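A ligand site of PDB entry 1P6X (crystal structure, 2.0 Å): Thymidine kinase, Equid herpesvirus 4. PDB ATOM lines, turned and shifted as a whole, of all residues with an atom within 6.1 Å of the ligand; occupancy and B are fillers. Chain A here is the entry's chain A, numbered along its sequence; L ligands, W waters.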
ATOM      1  N   TYR A  16     -11.219 -17.736 -22.375  1.00  0.00           N
ATOM      2  CA  TYR A  16     -10.632 -16.449 -22.676  1.00  0.00           C
ATOM      3  C   TYR A  16      -9.217 -16.609 -23.224  1.00  0.00           C
ATOM      4  O   TYR A  16      -8.474 -17.517 -22.855  1.00  0.00           O
ATOM      5  CB  TYR A  16     -10.662 -15.488 -21.455  1.00  0.00           C
ATOM      6  CG  TYR A  16      -9.784 -15.869 -20.304  1.00  0.00           C
ATOM      7  CD1 TYR A  16      -8.482 -15.362 -20.169  1.00  0.00           C
ATOM      8  CD2 TYR A  16     -10.261 -16.714 -19.302  1.00  0.00           C
ATOM      9  CE1 TYR A  16      -7.673 -15.715 -19.056  1.00  0.00           C
ATOM     10  CE2 TYR A  16      -9.490 -17.063 -18.210  1.00  0.00           C
ATOM     11  CZ  TYR A  16      -8.214 -16.565 -18.087  1.00  0.00           C
ATOM     12  OH  TYR A  16      -7.516 -16.954 -16.976  1.00  0.00           O
ATOM     13  N   LYS A  20     -11.355 -15.484 -29.850  1.00  0.00           N
ATOM     14  CA  LYS A  20     -12.784 -15.337 -30.150  1.00  0.00           C
ATOM     15  C   LYS A  20     -13.200 -13.907 -30.556  1.00  0.00           C
ATOM     16  O   LYS A  20     -13.833 -13.698 -31.619  1.00  0.00           O
ATOM     17  CB  LYS A  20     -13.564 -15.868 -28.938  1.00  0.00           C
ATOM     18  CG  LYS A  20     -14.945 -15.294 -28.649  1.00  0.00           C
ATOM     19  CD  LYS A  20     -15.515 -15.995 -27.385  1.00  0.00           C
ATOM     20  CE  LYS A  20     -14.872 -15.505 -26.061  1.00  0.00           C
ATOM     21  NZ  LYS A  20     -14.519 -14.054 -26.049  1.00  0.00           N
ATOM     22  N   GLU A  42     -18.021  -8.593 -25.828  1.00  0.00           N
ATOM     23  CA  GLU A  42     -18.105  -8.735 -24.364  1.00  0.00           C
ATOM     24  C   GLU A  42     -18.479  -7.393 -23.738  1.00  0.00           C
ATOM     25  O   GLU A  42     -18.012  -6.350 -24.178  1.00  0.00           O
ATOM     26  CB  GLU A  42     -16.786  -9.245 -23.760  1.00  0.00           C
ATOM     27  CG  GLU A  42     -16.569 -10.736 -23.949  1.00  0.00           C
ATOM     28  CD  GLU A  42     -15.311 -11.211 -23.259  1.00  0.00           C
ATOM     29  OE1 GLU A  42     -14.286 -10.499 -23.295  1.00  0.00           O
ATOM     30  OE2 GLU A  42     -15.345 -12.271 -22.626  1.00  0.00           O
ATOM     31  N   MET A  44     -17.590  -5.270 -21.676  1.00  0.00           N
ATOM     32  CA  MET A  44     -16.409  -4.904 -20.904  1.00  0.00           C
ATOM     33  C   MET A  44     -16.658  -3.723 -19.959  1.00  0.00           C
ATOM     34  O   MET A  44     -16.267  -3.790 -18.791  1.00  0.00           O
ATOM     35  CB  MET A  44     -15.247  -4.570 -21.840  1.00  0.00           C
ATOM     36  CG  MET A  44     -13.860  -4.916 -21.336  1.00  0.00           C
ATOM     37  SD  MET A  44     -13.631  -6.389 -20.374  1.00  0.00           S
ATOM     38  CE  MET A  44     -13.266  -7.606 -21.625  1.00  0.00           C
ATOM     39  N   TRP A  47     -18.779  -4.622 -16.942  1.00  0.00           N
ATOM     40  CA  TRP A  47     -17.927  -5.315 -15.991  1.00  0.00           C
ATOM     41  C   TRP A  47     -16.933  -4.421 -15.236  1.00  0.00           C
ATOM     42  O   TRP A  47     -16.658  -4.650 -14.042  1.00  0.00           O
ATOM     43  CB  TRP A  47     -17.148  -6.404 -16.709  1.00  0.00           C
ATOM     44  CG  TRP A  47     -17.984  -7.582 -17.177  1.00  0.00           C
ATOM     45  CD1 TRP A  47     -19.223  -7.947 -16.744  1.00  0.00           C
ATOM     46  CD2 TRP A  47     -17.610  -8.551 -18.158  1.00  0.00           C
ATOM     47  NE1 TRP A  47     -19.635  -9.093 -17.389  1.00  0.00           N
ATOM     48  CE2 TRP A  47     -18.672  -9.471 -18.279  1.00  0.00           C
ATOM     49  CE3 TRP A  47     -16.478  -8.729 -18.968  1.00  0.00           C
ATOM     50  CZ2 TRP A  47     -18.634 -10.576 -19.149  1.00  0.00           C
ATOM     51  CZ3 TRP A  47     -16.438  -9.820 -19.853  1.00  0.00           C
ATOM     52  CH2 TRP A  47     -17.518 -10.730 -19.935  1.00  0.00           C
ATOM     53  N   ILE A  56     -13.714  -7.925 -12.893  1.00  0.00           N
ATOM     54  CA  ILE A  56     -12.587  -8.749 -13.360  1.00  0.00           C
ATOM     55  C   ILE A  56     -11.451  -8.637 -12.355  1.00  0.00           C
ATOM     56  O   ILE A  56     -10.931  -9.655 -11.892  1.00  0.00           O
ATOM     57  CB  ILE A  56     -12.148  -8.398 -14.810  1.00  0.00           C
ATOM     58  CG1 ILE A  56     -13.122  -9.008 -15.820  1.00  0.00           C
ATOM     59  CG2 ILE A  56     -10.734  -8.940 -15.068  1.00  0.00           C
ATOM     60  CD1 ILE A  56     -13.237  -8.240 -17.134  1.00  0.00           C
ATOM     61  N   ILE A  59     -12.695 -10.389  -8.965  1.00  0.00           N
ATOM     62  CA  ILE A  59     -12.693 -11.847  -8.873  1.00  0.00           C
ATOM     63  C   ILE A  59     -11.269 -12.397  -8.772  1.00  0.00           C
ATOM     64  O   ILE A  59     -11.018 -13.312  -7.995  1.00  0.00           O
ATOM     65  CB  ILE A  59     -13.548 -12.517 -10.020  1.00  0.00           C
ATOM     66  CG1 ILE A  59     -13.989 -13.930  -9.603  1.00  0.00           C
ATOM     67  CG2 ILE A  59     -12.801 -12.534 -11.362  1.00  0.00           C
ATOM     68  CD1 ILE A  59     -15.240 -14.449 -10.284  1.00  0.00           C
ATOM     69  N   TYR A  60     -10.326 -11.827  -9.531  1.00  0.00           N
ATOM     70  CA  TYR A  60      -8.936 -12.254  -9.401  1.00  0.00           C
ATOM     71  C   TYR A  60      -8.322 -11.773  -8.074  1.00  0.00           C
ATOM     72  O   TYR A  60      -7.596 -12.514  -7.416  1.00  0.00           O
ATOM     73  CB  TYR A  60      -8.097 -11.861 -10.637  1.00  0.00           C
ATOM     74  CG  TYR A  60      -8.494 -12.622 -11.904  1.00  0.00           C
ATOM     75  CD1 TYR A  60      -9.130 -11.968 -12.969  1.00  0.00           C
ATOM     76  CD2 TYR A  60      -8.250 -13.998 -12.044  1.00  0.00           C
ATOM     77  CE1 TYR A  60      -9.502 -12.660 -14.138  1.00  0.00           C
ATOM     78  CE2 TYR A  60      -8.618 -14.700 -13.204  1.00  0.00           C
ATOM     79  CZ  TYR A  60      -9.248 -14.026 -14.249  1.00  0.00           C
ATOM     80  OH  TYR A  60      -9.605 -14.701 -15.395  1.00  0.00           O
ATOM     81  N   GLN A  84     -18.999 -13.662  -9.765  1.00  0.00           N
ATOM     82  CA  GLN A  84     -19.426 -14.492 -10.877  1.00  0.00           C
ATOM     83  C   GLN A  84     -20.858 -14.151 -11.259  1.00  0.00           C
ATOM     84  O   GLN A  84     -21.191 -14.132 -12.439  1.00  0.00           O
ATOM     85  CB  GLN A  84     -19.237 -15.968 -10.502  1.00  0.00           C
ATOM     86  CG  GLN A  84     -19.029 -16.984 -11.618  1.00  0.00           C
ATOM     87  CD  GLN A  84     -18.355 -16.428 -12.868  1.00  0.00           C
ATOM     88  OE1 GLN A  84     -17.135 -16.257 -12.905  1.00  0.00           O
ATOM     89  NE2 GLN A  84     -19.163 -16.155 -13.885  1.00  0.00           N
ATOM     90  N   PHE A  87     -20.865 -11.037 -13.452  1.00  0.00           N
ATOM     91  CA  PHE A  87     -20.462 -11.238 -14.837  1.00  0.00           C
ATOM     92  C   PHE A  87     -21.713 -11.462 -15.719  1.00  0.00           C
ATOM     93  O   PHE A  87     -21.750 -10.975 -16.841  1.00  0.00           O
ATOM     94  CB  PHE A  87     -19.528 -12.427 -15.000  1.00  0.00           C
ATOM     95  CG  PHE A  87     -18.076 -12.089 -14.810  1.00  0.00           C
ATOM     96  CD1 PHE A  87     -17.471 -12.313 -13.576  1.00  0.00           C
ATOM     97  CD2 PHE A  87     -17.331 -11.561 -15.847  1.00  0.00           C
ATOM     98  CE1 PHE A  87     -16.114 -12.020 -13.385  1.00  0.00           C
ATOM     99  CE2 PHE A  87     -15.994 -11.249 -15.669  1.00  0.00           C
ATOM    100  CZ  PHE A  87     -15.368 -11.492 -14.422  1.00  0.00           C
ATOM    101  N   THR A  88     -22.736 -12.152 -15.179  1.00  0.00           N
ATOM    102  CA  THR A  88     -23.874 -12.607 -15.991  1.00  0.00           C
ATOM    103  C   THR A  88     -24.838 -11.481 -16.355  1.00  0.00           C
ATOM    104  O   THR A  88     -25.501 -11.522 -17.373  1.00  0.00           O
ATOM    105  CB  THR A  88     -24.689 -13.690 -15.271  1.00  0.00           C
ATOM    106  OG1 THR A  88     -25.249 -13.125 -14.095  1.00  0.00           O
ATOM    107  CG2 THR A  88     -23.778 -14.792 -14.738  1.00  0.00           C
ATOM    108  N   TYR A  91     -25.131  -9.923 -19.838  1.00  0.00           N
ATOM    109  CA  TYR A  91     -25.569 -10.987 -20.766  1.00  0.00           C
ATOM    110  C   TYR A  91     -27.042 -11.268 -20.655  1.00  0.00           C
ATOM    111  O   TYR A  91     -27.700 -11.488 -21.665  1.00  0.00           O
ATOM    112  CB  TYR A  91     -24.781 -12.276 -20.517  1.00  0.00           C
ATOM    113  CG  TYR A  91     -23.444 -12.202 -21.180  1.00  0.00           C
ATOM    114  CD1 TYR A  91     -23.341 -12.360 -22.576  1.00  0.00           C
ATOM    115  CD2 TYR A  91     -22.289 -11.927 -20.452  1.00  0.00           C
ATOM    116  CE1 TYR A  91     -22.108 -12.261 -23.232  1.00  0.00           C
ATOM    117  CE2 TYR A  91     -21.030 -11.827 -21.118  1.00  0.00           C
ATOM    118  CZ  TYR A  91     -20.969 -11.994 -22.506  1.00  0.00           C
ATOM    119  OH  TYR A  91     -19.780 -11.904 -23.199  1.00  0.00           O
ATOM    120  N   ARG A 121     -19.835 -14.666 -26.709  1.00  0.00           N
ATOM    121  CA  ARG A 121     -20.356 -15.542 -25.646  1.00  0.00           C
ATOM    122  C   ARG A 121     -21.873 -15.623 -25.625  1.00  0.00           C
ATOM    123  O   ARG A 121     -22.562 -14.697 -26.030  1.00  0.00           O
ATOM    124  CB  ARG A 121     -19.813 -15.181 -24.247  1.00  0.00           C
ATOM    125  CG  ARG A 121     -18.292 -15.011 -24.140  1.00  0.00           C
ATOM    126  CD  ARG A 121     -17.785 -14.630 -22.692  1.00  0.00           C
ATOM    127  NE  ARG A 121     -16.311 -14.733 -22.613  1.00  0.00           N
ATOM    128  CZ  ARG A 121     -15.680 -15.899 -22.589  1.00  0.00           C
ATOM    129  NH1 ARG A 121     -16.381 -16.999 -22.635  1.00  0.00           N
ATOM    130  NH2 ARG A 121     -14.344 -15.967 -22.533  1.00  0.00           N
ATOM    131  N   ALA A 125     -21.892 -19.044 -20.656  1.00  0.00           N
ATOM    132  CA  ALA A 125     -20.490 -18.829 -20.251  1.00  0.00           C
ATOM    133  C   ALA A 125     -20.454 -18.392 -18.804  1.00  0.00           C
ATOM    134  O   ALA A 125     -19.726 -18.971 -17.991  1.00  0.00           O
ATOM    135  CB  ALA A 125     -19.814 -17.753 -21.127  1.00  0.00           C
ATOM    136  N   SER A 126     -21.268 -17.394 -18.466  1.00  0.00           N
ATOM    137  CA  SER A 126     -21.214 -16.768 -17.146  1.00  0.00           C
ATOM    138  C   SER A 126     -22.126 -17.439 -16.130  1.00  0.00           C
ATOM    139  O   SER A 126     -21.909 -17.338 -14.921  1.00  0.00           O
ATOM    140  CB  SER A 126     -21.470 -15.252 -17.263  1.00  0.00           C
ATOM    141  OG  SER A 126     -22.719 -14.950 -17.896  1.00  0.00           O
ATOM    142  N   THR A 127     -23.133 -18.177 -16.588  1.00  0.00           N
ATOM    143  CA  THR A 127     -24.044 -18.810 -15.627  1.00  0.00           C
ATOM    144  C   THR A 127     -23.661 -20.255 -15.356  1.00  0.00           C
ATOM    145  O   THR A 127     -24.057 -20.789 -14.332  1.00  0.00           O
ATOM    146  CB  THR A 127     -25.515 -18.755 -16.098  1.00  0.00           C
ATOM    147  OG1 THR A 127     -25.592 -19.312 -17.409  1.00  0.00           O
ATOM    148  CG2 THR A 127     -25.983 -17.293 -16.271  1.00  0.00           C
ATOM    149  N   PHE A 130     -18.013 -20.801 -16.382  1.00  0.00           N
ATOM    150  CA  PHE A 130     -17.077 -20.170 -15.454  1.00  0.00           C
ATOM    151  C   PHE A 130     -17.409 -20.515 -13.999  1.00  0.00           C
ATOM    152  O   PHE A 130     -16.495 -20.850 -13.259  1.00  0.00           O
ATOM    153  CB  PHE A 130     -16.997 -18.670 -15.688  1.00  0.00           C
ATOM    154  CG  PHE A 130     -16.046 -18.280 -16.822  1.00  0.00           C
ATOM    155  CD1 PHE A 130     -16.427 -18.422 -18.159  1.00  0.00           C
ATOM    156  CD2 PHE A 130     -14.788 -17.762 -16.538  1.00  0.00           C
ATOM    157  CE1 PHE A 130     -15.555 -18.052 -19.205  1.00  0.00           C
ATOM    158  CE2 PHE A 130     -13.905 -17.390 -17.575  1.00  0.00           C
ATOM    159  CZ  PHE A 130     -14.306 -17.529 -18.923  1.00  0.00           C
ATOM    160  N   PRO A 131     -18.681 -20.483 -13.597  1.00  0.00           N
ATOM    161  CA  PRO A 131     -19.069 -21.041 -12.286  1.00  0.00           C
ATOM    162  C   PRO A 131     -18.662 -22.486 -12.112  1.00  0.00           C
ATOM    163  O   PRO A 131     -18.174 -22.825 -11.032  1.00  0.00           O
ATOM    164  CB  PRO A 131     -20.595 -20.917 -12.298  1.00  0.00           C
ATOM    165  CG  PRO A 131     -20.851 -19.734 -13.129  1.00  0.00           C
ATOM    166  CD  PRO A 131     -19.841 -19.868 -14.285  1.00  0.00           C
ATOM    167  N   ARG A 134     -14.879 -22.568 -11.486  1.00  0.00           N
ATOM    168  CA  ARG A 134     -14.618 -22.095 -10.116  1.00  0.00           C
ATOM    169  C   ARG A 134     -14.976 -23.116  -9.042  1.00  0.00           C
ATOM    170  O   ARG A 134     -14.234 -23.272  -8.066  1.00  0.00           O
ATOM    171  CB  ARG A 134     -15.312 -20.761  -9.853  1.00  0.00           C
ATOM    172  CG  ARG A 134     -14.807 -19.582 -10.708  1.00  0.00           C
ATOM    173  CD  ARG A 134     -13.449 -19.069 -10.274  1.00  0.00           C
ATOM    174  NE  ARG A 134     -12.959 -17.955 -11.073  1.00  0.00           N
ATOM    175  CZ  ARG A 134     -11.755 -17.434 -10.937  1.00  0.00           C
ATOM    176  NH1 ARG A 134     -10.917 -17.910 -10.014  1.00  0.00           N
ATOM    177  NH2 ARG A 134     -11.374 -16.420 -11.702  1.00  0.00           N
ATOM    178  N   LEU A 193     -11.101 -24.583 -17.412  1.00  0.00           N
ATOM    179  CA  LEU A 193     -12.090 -23.943 -18.310  1.00  0.00           C
ATOM    180  C   LEU A 193     -12.100 -24.635 -19.665  1.00  0.00           C
ATOM    181  O   LEU A 193     -13.141 -24.841 -20.235  1.00  0.00           O
ATOM    182  CB  LEU A 193     -11.812 -22.454 -18.520  1.00  0.00           C
ATOM    183  CG  LEU A 193     -12.260 -21.476 -17.408  1.00  0.00           C
ATOM    184  CD1 LEU A 193     -11.627 -20.101 -17.610  1.00  0.00           C
ATOM    185  CD2 LEU A 193     -13.817 -21.350 -17.339  1.00  0.00           C
HETATM  186  O1  LIG L   1     -13.488 -12.704 -20.387  1.00  0.00           O
HETATM  187  C1  LIG L   1     -12.969 -11.528 -19.775  1.00  0.00           C
HETATM  188  C2  LIG L   1     -12.356 -11.850 -18.413  1.00  0.00           C
HETATM  189  O2  LIG L   1     -13.413 -12.170 -17.495  1.00  0.00           O
HETATM  190  C3  LIG L   1     -11.402 -13.048 -18.397  1.00  0.00           C
HETATM  191  O3  LIG L   1     -10.343 -12.774 -17.477  1.00  0.00           O
HETATM  192  C4  LIG L   1     -12.241 -14.185 -17.835  1.00  0.00           C
HETATM  193  C5  LIG L   1     -13.253 -13.466 -16.943  1.00  0.00           C
HETATM  194  N1  LIG L   1     -14.597 -14.053 -16.895  1.00  0.00           N
HETATM  195  C6  LIG L   1     -15.033 -14.635 -15.677  1.00  0.00           C
HETATM  196  O4  LIG L   1     -14.246 -14.703 -14.688  1.00  0.00           O
HETATM  197  N2  LIG L   1     -16.264 -15.129 -15.553  1.00  0.00           N
HETATM  198  C7  LIG L   1     -17.139 -15.093 -16.584  1.00  0.00           C
HETATM  199  O5  LIG L   1     -18.261 -15.589 -16.389  1.00  0.00           O
HETATM  200  C8  LIG L   1     -16.741 -14.492 -17.884  1.00  0.00           C
HETATM  201  C9  LIG L   1     -17.660 -14.427 -19.093  1.00  0.00           C
HETATM  202  C10 LIG L   1     -15.443 -13.961 -17.963  1.00  0.00           C
HETATM  203  O   HOH W   1     -12.026 -15.999 -14.358  1.00  0.00           O
HETATM  204  O   HOH W   2     -14.597 -17.062 -12.826  1.00  0.00           O
HETATM  205  O   HOH W   3      -8.214 -11.360 -18.119  1.00  0.00           O
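Tyr 16 touches the ligand (CD2 to C4, 3.5 Å). Trp 47 touches the ligand (CH2 to C9, 3.8 Å). CG1 of Ile 56 touches O2 of the ligand, 3.6 Å away. Phe 87 touches the ligand. Arg 121 touches the ligand. Ser 126 touches the ligand. Phe 130 touches the ligand (CD2 to N2, 3.2 Å). Hydrophobic or aromatic side chains that line the ligand: Tyr 16, Trp 47, Ile 56, Tyr 60, Phe 87 and Phe 130. Ten residues have an atom within 4 Å of the ligand: Tyr 16, Glu 42, Trp 47, Ile 56, Tyr 60, Gln 84, Phe 87, Arg 121, Ser 126 and Phe 130. Along chain A the residues within 4 Å of the ligand span positions 16 to 130.
NE2 of Gln 84 is in hydrogen-bond range of O5 of the ligand, at 2.7 Å. The side-chain hydroxyl (OH) of Tyr 60 is in hydrogen-bond range of an oxygen (O3) of the ligand, at 2.9 Å. The side-chain carboxylate of Glu 42 lies within hydrogen-bond range of an oxygen (O1) of the ligand (2.9 Å).
The side-chain amide nitrogen (NE2) of Gln 84 sits at hydrogen-bond distance from the backbone carbonyl oxygen (O) of Ser 126, 3.2 Å away. OH of Tyr 16 sits at hydrogen-bond distance from OH of Tyr 60 (3.5 Å). The side-chain carboxylate (OE2) of Glu 42 lies within salt-bridge range of the guanidinium group (NE) of Arg 121 (2.6 Å). OE2 of Glu 42 is in salt-bridge range of NZ of Lys 20 (3.9 Å). N of Phe 130 lies within hydrogen-bond range of O of Ala 125 (3.0 Å). O of Phe 87 lies within hydrogen-bond range of NE1 of Trp 47, at 2.9 Å.
Water W1 lies within hydrogen-bond range of an oxygen (O4) of the ligand, the guanidinium group of Arg 134 and the side-chain hydroxyl of Tyr 60. Water W2 lies within hydrogen-bond range of the guanidinium group (NE) of Arg 134 (2.6 Å), the side-chain amide oxygen (OE1) of Gln 84 (2.7 Å) and an oxygen (O4) of the ligand (3.0 Å).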
